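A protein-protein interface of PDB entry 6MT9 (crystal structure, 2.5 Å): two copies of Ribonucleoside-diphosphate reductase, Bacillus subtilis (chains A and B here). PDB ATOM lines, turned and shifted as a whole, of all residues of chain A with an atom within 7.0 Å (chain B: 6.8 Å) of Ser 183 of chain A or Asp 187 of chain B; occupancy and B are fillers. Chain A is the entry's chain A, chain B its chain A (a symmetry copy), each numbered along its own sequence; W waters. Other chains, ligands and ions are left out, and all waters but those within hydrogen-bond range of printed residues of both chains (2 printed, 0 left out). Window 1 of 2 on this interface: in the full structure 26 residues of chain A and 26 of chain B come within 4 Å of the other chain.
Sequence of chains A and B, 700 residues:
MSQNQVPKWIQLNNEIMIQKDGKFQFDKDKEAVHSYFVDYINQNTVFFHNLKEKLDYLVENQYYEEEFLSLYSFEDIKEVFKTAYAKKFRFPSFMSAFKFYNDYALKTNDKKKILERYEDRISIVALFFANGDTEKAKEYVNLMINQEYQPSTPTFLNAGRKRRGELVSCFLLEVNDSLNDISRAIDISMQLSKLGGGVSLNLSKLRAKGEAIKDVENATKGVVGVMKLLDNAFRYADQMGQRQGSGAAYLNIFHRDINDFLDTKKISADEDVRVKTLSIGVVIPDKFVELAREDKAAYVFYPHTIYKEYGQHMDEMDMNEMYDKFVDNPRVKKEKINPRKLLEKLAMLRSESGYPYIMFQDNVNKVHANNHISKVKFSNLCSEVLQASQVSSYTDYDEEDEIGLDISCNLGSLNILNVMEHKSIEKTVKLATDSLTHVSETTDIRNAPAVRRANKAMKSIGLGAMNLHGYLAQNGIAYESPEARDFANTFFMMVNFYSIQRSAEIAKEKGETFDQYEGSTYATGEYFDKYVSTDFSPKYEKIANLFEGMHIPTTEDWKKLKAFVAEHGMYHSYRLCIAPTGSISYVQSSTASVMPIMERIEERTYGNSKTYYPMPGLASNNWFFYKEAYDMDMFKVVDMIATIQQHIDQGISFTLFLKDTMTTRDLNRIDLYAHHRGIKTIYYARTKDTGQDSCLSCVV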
ATOM      1  N   VAL A 175      14.644 -21.686  -7.170  1.00  0.00           N
ATOM      2  CA  VAL A 175      15.164 -22.117  -8.468  1.00  0.00           C
ATOM      3  C   VAL A 175      15.659 -23.552  -8.350  1.00  0.00           C
ATOM      4  O   VAL A 175      16.546 -23.843  -7.540  1.00  0.00           O
ATOM      5  CB  VAL A 175      16.299 -21.209  -8.972  1.00  0.00           C
ATOM      6  CG1 VAL A 175      16.656 -21.574 -10.407  1.00  0.00           C
ATOM      7  CG2 VAL A 175      15.922 -19.731  -8.855  1.00  0.00           C
ATOM      8  N   SER A 178      18.037 -27.359 -12.741  1.00  0.00           N
ATOM      9  CA  SER A 178      17.970 -27.794 -14.133  1.00  0.00           C
ATOM     10  C   SER A 178      18.015 -26.582 -15.046  1.00  0.00           C
ATOM     11  O   SER A 178      17.672 -25.465 -14.647  1.00  0.00           O
ATOM     12  CB  SER A 178      16.701 -28.603 -14.433  1.00  0.00           C
ATOM     13  OG  SER A 178      15.616 -27.737 -14.721  1.00  0.00           O
ATOM     14  N   LEU A 179      18.421 -26.821 -16.296  1.00  0.00           N
ATOM     15  CA  LEU A 179      18.395 -25.755 -17.292  1.00  0.00           C
ATOM     16  C   LEU A 179      16.975 -25.226 -17.504  1.00  0.00           C
ATOM     17  O   LEU A 179      16.764 -24.008 -17.567  1.00  0.00           O
ATOM     18  CB  LEU A 179      19.005 -26.255 -18.606  1.00  0.00           C
ATOM     19  CG  LEU A 179      19.081 -25.258 -19.764  1.00  0.00           C
ATOM     20  CD1 LEU A 179      19.879 -24.014 -19.373  1.00  0.00           C
ATOM     21  CD2 LEU A 179      19.675 -25.912 -20.993  1.00  0.00           C
ATOM     22  N   ASN A 180      15.985 -26.126 -17.590  1.00  0.00           N
ATOM     23  CA  ASN A 180      14.585 -25.709 -17.676  1.00  0.00           C
ATOM     24  C   ASN A 180      14.228 -24.707 -16.580  1.00  0.00           C
ATOM     25  O   ASN A 180      13.608 -23.668 -16.845  1.00  0.00           O
ATOM     26  CB  ASN A 180      13.654 -26.921 -17.574  1.00  0.00           C
ATOM     27  CG  ASN A 180      13.728 -27.840 -18.779  1.00  0.00           C
ATOM     28  OD1 ASN A 180      14.201 -27.460 -19.852  1.00  0.00           O
ATOM     29  ND2 ASN A 180      13.231 -29.062 -18.607  1.00  0.00           N
ATOM     30  N   ASP A 181      14.601 -25.016 -15.335  1.00  0.00           N
ATOM     31  CA  ASP A 181      14.233 -24.150 -14.219  1.00  0.00           C
ATOM     32  C   ASP A 181      14.988 -22.835 -14.274  1.00  0.00           C
ATOM     33  O   ASP A 181      14.426 -21.776 -13.964  1.00  0.00           O
ATOM     34  CB  ASP A 181      14.488 -24.865 -12.891  1.00  0.00           C
ATOM     35  CG  ASP A 181      13.536 -26.023 -12.670  1.00  0.00           C
ATOM     36  OD1 ASP A 181      12.319 -25.773 -12.543  1.00  0.00           O
ATOM     37  OD2 ASP A 181      14.000 -27.186 -12.651  1.00  0.00           O
ATOM     38  N   ILE A 182      16.262 -22.884 -14.663  1.00  0.00           N
ATOM     39  CA  ILE A 182      17.045 -21.665 -14.801  1.00  0.00           C
ATOM     40  C   ILE A 182      16.417 -20.746 -15.837  1.00  0.00           C
ATOM     41  O   ILE A 182      16.300 -19.534 -15.618  1.00  0.00           O
ATOM     42  CB  ILE A 182      18.502 -22.012 -15.150  1.00  0.00           C
ATOM     43  CG1 ILE A 182      19.144 -22.734 -13.972  1.00  0.00           C
ATOM     44  CG2 ILE A 182      19.284 -20.759 -15.554  1.00  0.00           C
ATOM     45  CD1 ILE A 182      20.498 -23.259 -14.277  1.00  0.00           C
ATOM     46  N   SER A 183      15.980 -21.309 -16.973  1.00  0.00           N
ATOM     47  CA  SER A 183      15.343 -20.492 -18.006  1.00  0.00           C
ATOM     48  C   SER A 183      14.048 -19.872 -17.505  1.00  0.00           C
ATOM     49  O   SER A 183      13.751 -18.711 -17.800  1.00  0.00           O
ATOM     50  CB  SER A 183      15.070 -21.329 -19.252  1.00  0.00           C
ATOM     51  OG  SER A 183      16.279 -21.683 -19.867  1.00  0.00           O
ATOM     52  N   ARG A 184      13.257 -20.637 -16.753  1.00  0.00           N
ATOM     53  CA  ARG A 184      12.008 -20.099 -16.227  1.00  0.00           C
ATOM     54  C   ARG A 184      12.265 -19.006 -15.193  1.00  0.00           C
ATOM     55  O   ARG A 184      11.521 -18.021 -15.131  1.00  0.00           O
ATOM     56  CB  ARG A 184      11.169 -21.236 -15.640  1.00  0.00           C
ATOM     57  CG  ARG A 184       9.880 -20.788 -15.004  1.00  0.00           C
ATOM     58  CD  ARG A 184       8.996 -20.104 -15.997  1.00  0.00           C
ATOM     59  NE  ARG A 184       8.531 -21.028 -17.020  1.00  0.00           N
ATOM     60  CZ  ARG A 184       7.747 -20.671 -18.026  1.00  0.00           C
ATOM     61  NH1 ARG A 184       7.345 -19.408 -18.131  1.00  0.00           N
ATOM     62  NH2 ARG A 184       7.364 -21.571 -18.918  1.00  0.00           N
ATOM     63  N   ALA A 185      13.318 -19.150 -14.383  1.00  0.00           N
ATOM     64  CA  ALA A 185      13.631 -18.120 -13.393  1.00  0.00           C
ATOM     65  C   ALA A 185      14.077 -16.826 -14.066  1.00  0.00           C
ATOM     66  O   ALA A 185      13.723 -15.729 -13.612  1.00  0.00           O
ATOM     67  CB  ALA A 185      14.699 -18.626 -12.421  1.00  0.00           C
ATOM     68  N   ILE A 186      14.841 -16.934 -15.159  1.00  0.00           N
ATOM     69  CA  ILE A 186      15.215 -15.755 -15.945  1.00  0.00           C
ATOM     70  C   ILE A 186      13.968 -15.024 -16.427  1.00  0.00           C
ATOM     71  O   ILE A 186      13.844 -13.802 -16.285  1.00  0.00           O
ATOM     72  CB  ILE A 186      16.107 -16.158 -17.133  1.00  0.00           C
ATOM     73  CG1 ILE A 186      17.418 -16.780 -16.655  1.00  0.00           C
ATOM     74  CG2 ILE A 186      16.380 -14.963 -18.021  1.00  0.00           C
ATOM     75  CD1 ILE A 186      18.168 -17.492 -17.774  1.00  0.00           C
ATOM     76  N   ASP A 187      13.021 -15.762 -16.999  1.00  0.00           N
ATOM     77  CA  ASP A 187      11.821 -15.116 -17.511  1.00  0.00           C
ATOM     78  C   ASP A 187      10.971 -14.539 -16.381  1.00  0.00           C
ATOM     79  O   ASP A 187      10.485 -13.407 -16.482  1.00  0.00           O
ATOM     80  CB  ASP A 187      11.009 -16.092 -18.359  1.00  0.00           C
ATOM     81  CG  ASP A 187       9.685 -15.504 -18.791  1.00  0.00           C
ATOM     82  OD1 ASP A 187       9.678 -14.352 -19.276  1.00  0.00           O
ATOM     83  OD2 ASP A 187       8.648 -16.172 -18.625  1.00  0.00           O
ATOM     84  N   ILE A 188      10.763 -15.303 -15.302  1.00  0.00           N
ATOM     85  CA  ILE A 188       9.954 -14.787 -14.195  1.00  0.00           C
ATOM     86  C   ILE A 188      10.569 -13.503 -13.656  1.00  0.00           C
ATOM     87  O   ILE A 188       9.880 -12.491 -13.478  1.00  0.00           O
ATOM     88  CB  ILE A 188       9.800 -15.840 -13.084  1.00  0.00           C
ATOM     89  CG1 ILE A 188       8.939 -17.016 -13.539  1.00  0.00           C
ATOM     90  CG2 ILE A 188       9.182 -15.215 -11.845  1.00  0.00           C
ATOM     91  CD1 ILE A 188       9.070 -18.245 -12.628  1.00  0.00           C
ATOM     92  N   LEU A 229      23.604 -14.662 -16.019  1.00  0.00           N
ATOM     93  CA  LEU A 229      22.362 -14.621 -16.789  1.00  0.00           C
ATOM     94  C   LEU A 229      21.331 -13.723 -16.114  1.00  0.00           C
ATOM     95  O   LEU A 229      20.695 -12.889 -16.768  1.00  0.00           O
ATOM     96  CB  LEU A 229      21.811 -16.041 -16.975  1.00  0.00           C
ATOM     97  CG  LEU A 229      22.604 -17.000 -17.873  1.00  0.00           C
ATOM     98  CD1 LEU A 229      22.082 -18.429 -17.764  1.00  0.00           C
ATOM     99  CD2 LEU A 229      22.552 -16.536 -19.310  1.00  0.00           C
ATOM    100  N   TYR A 397       8.892 -28.847 -22.377  1.00  0.00           N
ATOM    101  CA  TYR A 397       7.779 -28.071 -22.913  1.00  0.00           C
ATOM    102  C   TYR A 397       6.496 -28.893 -22.995  1.00  0.00           C
ATOM    103  O   TYR A 397       5.410 -28.386 -22.688  1.00  0.00           O
ATOM    104  CB  TYR A 397       8.155 -27.511 -24.286  1.00  0.00           C
ATOM    105  CG  TYR A 397       7.073 -26.665 -24.902  1.00  0.00           C
ATOM    106  CD1 TYR A 397       6.186 -27.196 -25.844  1.00  0.00           C
ATOM    107  CD2 TYR A 397       6.922 -25.338 -24.537  1.00  0.00           C
ATOM    108  CE1 TYR A 397       5.179 -26.420 -26.404  1.00  0.00           C
ATOM    109  CE2 TYR A 397       5.917 -24.552 -25.090  1.00  0.00           C
ATOM    110  CZ  TYR A 397       5.048 -25.097 -26.016  1.00  0.00           C
ATOM    111  OH  TYR A 397       4.060 -24.304 -26.554  1.00  0.00           O
ATOM    112  N   ILE B 182      10.918 -13.448 -26.497  1.00  0.00           N
ATOM    113  CA  ILE B 182      12.348 -13.299 -26.266  1.00  0.00           C
ATOM    114  C   ILE B 182      12.827 -14.310 -25.236  1.00  0.00           C
ATOM    115  O   ILE B 182      13.872 -14.948 -25.416  1.00  0.00           O
ATOM    116  CB  ILE B 182      12.663 -11.855 -25.843  1.00  0.00           C
ATOM    117  CG1 ILE B 182      12.374 -10.914 -27.005  1.00  0.00           C
ATOM    118  CG2 ILE B 182      14.106 -11.730 -25.346  1.00  0.00           C
ATOM    119  CD1 ILE B 182      12.488  -9.481 -26.639  1.00  0.00           C
ATOM    120  N   SER B 183      12.062 -14.491 -24.151  1.00  0.00           N
ATOM    121  CA  SER B 183      12.446 -15.465 -23.129  1.00  0.00           C
ATOM    122  C   SER B 183      12.455 -16.880 -23.683  1.00  0.00           C
ATOM    123  O   SER B 183      13.344 -17.675 -23.363  1.00  0.00           O
ATOM    124  CB  SER B 183      11.501 -15.381 -21.933  1.00  0.00           C
ATOM    125  OG  SER B 183      11.685 -14.165 -21.260  1.00  0.00           O
ATOM    126  N   ARG B 184      11.465 -17.218 -24.509  1.00  0.00           N
ATOM    127  CA  ARG B 184      11.423 -18.554 -25.090  1.00  0.00           C
ATOM    128  C   ARG B 184      12.577 -18.774 -26.064  1.00  0.00           C
ATOM    129  O   ARG B 184      13.130 -19.877 -26.134  1.00  0.00           O
ATOM    130  CB  ARG B 184      10.070 -18.775 -25.769  1.00  0.00           C
ATOM    131  CG  ARG B 184       9.936 -20.103 -26.464  1.00  0.00           C
ATOM    132  CD  ARG B 184      10.095 -21.236 -25.501  1.00  0.00           C
ATOM    133  NE  ARG B 184       9.000 -21.276 -24.544  1.00  0.00           N
ATOM    134  CZ  ARG B 184       8.910 -22.175 -23.575  1.00  0.00           C
ATOM    135  NH1 ARG B 184       9.855 -23.102 -23.447  1.00  0.00           N
ATOM    136  NH2 ARG B 184       7.882 -22.148 -22.742  1.00  0.00           N
ATOM    137  N   ALA B 185      12.966 -17.738 -26.815  1.00  0.00           N
ATOM    138  CA  ALA B 185      14.085 -17.881 -27.745  1.00  0.00           C
ATOM    139  C   ALA B 185      15.399 -18.086 -26.997  1.00  0.00           C
ATOM    140  O   ALA B 185      16.250 -18.875 -27.430  1.00  0.00           O
ATOM    141  CB  ALA B 185      14.166 -16.664 -28.668  1.00  0.00           C
ATOM    142  N   ILE B 186      15.575 -17.395 -25.864  1.00  0.00           N
ATOM    143  CA  ILE B 186      16.748 -17.618 -25.014  1.00  0.00           C
ATOM    144  C   ILE B 186      16.819 -19.077 -24.581  1.00  0.00           C
ATOM    145  O   ILE B 186      17.864 -19.729 -24.684  1.00  0.00           O
ATOM    146  CB  ILE B 186      16.712 -16.684 -23.790  1.00  0.00           C
ATOM    147  CG1 ILE B 186      16.767 -15.217 -24.211  1.00  0.00           C
ATOM    148  CG2 ILE B 186      17.848 -17.008 -22.843  1.00  0.00           C
ATOM    149  CD1 ILE B 186      16.397 -14.270 -23.076  1.00  0.00           C
ATOM    150  N   ASP B 187      15.704 -19.615 -24.096  1.00  0.00           N
ATOM    151  CA  ASP B 187      15.717 -20.996 -23.633  1.00  0.00           C
ATOM    152  C   ASP B 187      15.923 -21.970 -24.790  1.00  0.00           C
ATOM    153  O   ASP B 187      16.713 -22.915 -24.677  1.00  0.00           O
ATOM    154  CB  ASP B 187      14.432 -21.318 -22.873  1.00  0.00           C
ATOM    155  CG  ASP B 187      14.344 -22.780 -22.501  1.00  0.00           C
ATOM    156  OD1 ASP B 187      15.341 -23.318 -21.974  1.00  0.00           O
ATOM    157  OD2 ASP B 187      13.296 -23.402 -22.754  1.00  0.00           O
ATOM    158  N   ILE B 188      15.213 -21.775 -25.908  1.00  0.00           N
ATOM    159  CA  ILE B 188      15.382 -22.687 -27.042  1.00  0.00           C
ATOM    160  C   ILE B 188      16.836 -22.690 -27.494  1.00  0.00           C
ATOM    161  O   ILE B 188      17.446 -23.752 -27.676  1.00  0.00           O
ATOM    162  CB  ILE B 188      14.440 -22.313 -28.199  1.00  0.00           C
ATOM    163  CG1 ILE B 188      12.979 -22.574 -27.841  1.00  0.00           C
ATOM    164  CG2 ILE B 188      14.799 -23.097 -29.449  1.00  0.00           C
ATOM    165  CD1 ILE B 188      11.993 -21.874 -28.788  1.00  0.00           C
ATOM    166  N   SER B 189      17.421 -21.498 -27.649  1.00  0.00           N
ATOM    167  CA  SER B 189      18.830 -21.400 -28.014  1.00  0.00           C
ATOM    168  C   SER B 189      19.695 -22.238 -27.085  1.00  0.00           C
ATOM    169  O   SER B 189      20.581 -22.968 -27.541  1.00  0.00           O
ATOM    170  CB  SER B 189      19.280 -19.943 -27.985  1.00  0.00           C
ATOM    171  OG  SER B 189      18.515 -19.164 -28.889  1.00  0.00           O
ATOM    172  N   MET B 190      19.429 -22.172 -25.779  1.00  0.00           N
ATOM    173  CA  MET B 190      20.228 -22.948 -24.842  1.00  0.00           C
ATOM    174  C   MET B 190      19.905 -24.430 -24.940  1.00  0.00           C
ATOM    175  O   MET B 190      20.795 -25.272 -24.774  1.00  0.00           O
ATOM    176  CB  MET B 190      20.021 -22.445 -23.413  1.00  0.00           C
ATOM    177  CG  MET B 190      20.574 -21.053 -23.175  1.00  0.00           C
ATOM    178  SD  MET B 190      20.812 -20.636 -21.437  1.00  0.00           S
ATOM    179  CE  MET B 190      19.149 -20.803 -20.790  1.00  0.00           C
ATOM    180  N   GLN B 191      18.641 -24.776 -25.190  1.00  0.00           N
ATOM    181  CA  GLN B 191      18.289 -26.190 -25.266  1.00  0.00           C
ATOM    182  C   GLN B 191      18.971 -26.846 -26.454  1.00  0.00           C
ATOM    183  O   GLN B 191      19.492 -27.961 -26.338  1.00  0.00           O
ATOM    184  CB  GLN B 191      16.771 -26.372 -25.362  1.00  0.00           C
ATOM    185  CG  GLN B 191      15.975 -25.854 -24.179  1.00  0.00           C
ATOM    186  CD  GLN B 191      16.142 -26.675 -22.914  1.00  0.00           C
ATOM    187  OE1 GLN B 191      16.540 -27.839 -22.945  1.00  0.00           O
ATOM    188  NE2 GLN B 191      15.824 -26.064 -21.787  1.00  0.00           N
ATOM    189  N   LEU B 192      18.985 -26.159 -27.599  1.00  0.00           N
ATOM    190  CA  LEU B 192      19.641 -26.689 -28.789  1.00  0.00           C
ATOM    191  C   LEU B 192      21.157 -26.638 -28.652  1.00  0.00           C
ATOM    192  O   LEU B 192      21.852 -27.589 -29.025  1.00  0.00           O
ATOM    193  CB  LEU B 192      19.195 -25.899 -30.020  1.00  0.00           C
ATOM    194  CG  LEU B 192      17.694 -25.908 -30.301  1.00  0.00           C
ATOM    195  CD1 LEU B 192      17.338 -24.939 -31.433  1.00  0.00           C
ATOM    196  CD2 LEU B 192      17.256 -27.330 -30.628  1.00  0.00           C
ATOM    197  N   SER B 193      21.683 -25.528 -28.133  1.00  0.00           N
ATOM    198  CA  SER B 193      23.123 -25.382 -27.976  1.00  0.00           C
ATOM    199  C   SER B 193      23.683 -26.413 -27.008  1.00  0.00           C
ATOM    200  O   SER B 193      24.816 -26.874 -27.177  1.00  0.00           O
ATOM    201  CB  SER B 193      23.446 -23.960 -27.510  1.00  0.00           C
ATOM    202  OG  SER B 193      24.765 -23.866 -27.002  1.00  0.00           O
ATOM    203  N   LEU B 230      21.128 -13.109 -25.728  1.00  0.00           N
ATOM    204  CA  LEU B 230      21.468 -14.323 -26.468  1.00  0.00           C
ATOM    205  C   LEU B 230      22.953 -14.637 -26.359  1.00  0.00           C
ATOM    206  O   LEU B 230      23.340 -15.796 -26.169  1.00  0.00           O
ATOM    207  CB  LEU B 230      21.068 -14.173 -27.932  1.00  0.00           C
ATOM    208  CG  LEU B 230      19.575 -14.127 -28.220  1.00  0.00           C
ATOM    209  CD1 LEU B 230      19.356 -13.563 -29.609  1.00  0.00           C
ATOM    210  CD2 LEU B 230      18.973 -15.523 -28.087  1.00  0.00           C
ATOM    211  N   ALA B 233      23.371 -16.379 -23.235  1.00  0.00           N
ATOM    212  CA  ALA B 233      22.785 -17.714 -23.270  1.00  0.00           C
ATOM    213  C   ALA B 233      23.735 -18.708 -23.930  1.00  0.00           C
ATOM    214  O   ALA B 233      23.967 -19.804 -23.407  1.00  0.00           O
ATOM    215  CB  ALA B 233      21.441 -17.672 -23.995  1.00  0.00           C
ATOM    216  N   ASN B 447      11.866 -29.468 -26.332  1.00  0.00           N
ATOM    217  CA  ASN B 447      12.111 -28.106 -25.865  1.00  0.00           C
ATOM    218  C   ASN B 447      12.350 -27.122 -27.011  1.00  0.00           C
ATOM    219  O   ASN B 447      12.873 -26.025 -26.786  1.00  0.00           O
ATOM    220  CB  ASN B 447      13.279 -28.076 -24.869  1.00  0.00           C
ATOM    221  CG  ASN B 447      12.962 -28.817 -23.578  1.00  0.00           C
ATOM    222  OD1 ASN B 447      11.820 -28.824 -23.118  1.00  0.00           O
ATOM    223  ND2 ASN B 447      13.969 -29.441 -22.990  1.00  0.00           N
HETATM  224  O   HOH W   1      12.443 -25.241 -21.020  1.00  0.00           O
HETATM  225  O   HOH W   2      16.439 -29.528 -20.534  1.00  0.00           O
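Ser 183 of chain A touches Asp 187 of chain B, and with the chains exchanged Asp 187 of chain A touches Ser 183 of chain B. Arg 184 of chain B touches its own counterpart, Arg 184 of chain A. 7 positions are printed for both chains. Of the 10 pairs that touch across the chains among the printed residues, 3 have their exchanged pair printed and touching as well.
Water W1 lies within hydrogen-bond range of OD2 of Asp 187 of chain B (2.7 Å) and OD1 of Asn 180 of chain A (3.1 Å). Water W2 lies within hydrogen-bond range of OE1 of Gln 191 of chain B (2.9 Å), OD1 of Asn 180 of chain A (3.1 Å) and ND2 of Asn 447 of chain B (3.5 Å).
N of Tyr 397 of chain A is in hydrogen-bond range of OD1 of Asn 447 of chain B, 3.0 Å away. OD1 of Asn 180 of chain A lies within hydrogen-bond range of NE2 of Gln 191 of chain B. OD1 of Asp 187 of chain A is in hydrogen-bond range of OG of Ser 183 of chain B, 2.8 Å away. The side-chain carboxylate (OD1) of Asp 187 of chain B sits at hydrogen-bond distance from the side-chain hydroxyl (OG) of Ser 183 of chain A (2.8 Å).
Of the 14 printed residues of chain A, 6 touch a printed residue of chain B. Hydrophobic or aromatic side chains of chain A within 4 Å of the printed part of chain B: Leu 179 and Tyr 397. Hydrophobic or aromatic side chains of chain B within 4 Å of the printed part of chain A: Met 190. Along chain B the printed residues that touch a printed residue of chain A span positions 183 to 447. Among the printed residues, 10 pairs touch across the chains. Among the printed residues, no Asp or Glu carboxylate lies within 4 Å of a Lys or Arg side-chain nitrogen of the other chain.
The guanidinium group (NH1) of Arg 184 of chain A lies within salt-bridge range of the side-chain carboxylate (OD2) of Asp 187 of chain A (3.5 Å). The side-chain hydroxyl (OG) of Ser 178 of chain A sits close to the backbone NH (N) of Asn 180 of chain A (3.3 Å). The side-chain hydroxyl of Ser 183 of chain A sits at hydrogen-bond distance from the backbone carbonyl oxygen of Leu 179 of chain A (3.3 Å). The guanidinium group of Arg 184 of chain B is in salt-bridge range of the side-chain carboxylate of Asp 187 of chain B, 3.5 Å away. OE1 of Gln 191 of chain B is in hydrogen-bond range of ND2 of Asn 447 of chain B (3.0 Å). The side-chain carboxylate (OD1) of Asp 187 of chain B lies within hydrogen-bond range of the side-chain amide nitrogen (NE2) of Gln 191 of chain B (2.8 Å).
Printed residues of chain B within 4 Å of Leu 179 of chain A: Met 190 (3.6 Å) and Gln 191 (3.9 Å). Of chain B, only Asp 187 (2.8 Å) and Met 190 (3.1 Å) come within 4 Å of Ser 183 of chain A. Of chain A, only Ser 183 (2.8 Å) comes within 4 Å of Asp 187 of chain B. Of the printed residues of chain A, Gln 191 of chain B touches Leu 179 and Asn 180. The nearest residue of chain A that does not touch Asp 187 of chain B is Leu 179 of chain A (4.7 Å). The nearest printed residue of chain B that does not touch Asp 187 of chain A is Arg 184 of chain B (6.2 Å).
Among the printed residues, pairs that only touch across the chains: Ser 183 of chain A with Met 190 of chain B, Leu 179 of chain A with Met 190 of chain B, Asn 180 of chain A with Asn 447 of chain B, Tyr 397 of chain A with Arg 184 of chain B, Arg 184 of chain A with Arg 184 of chain B and Leu 179 of chain A with Gln 191 of chain B.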
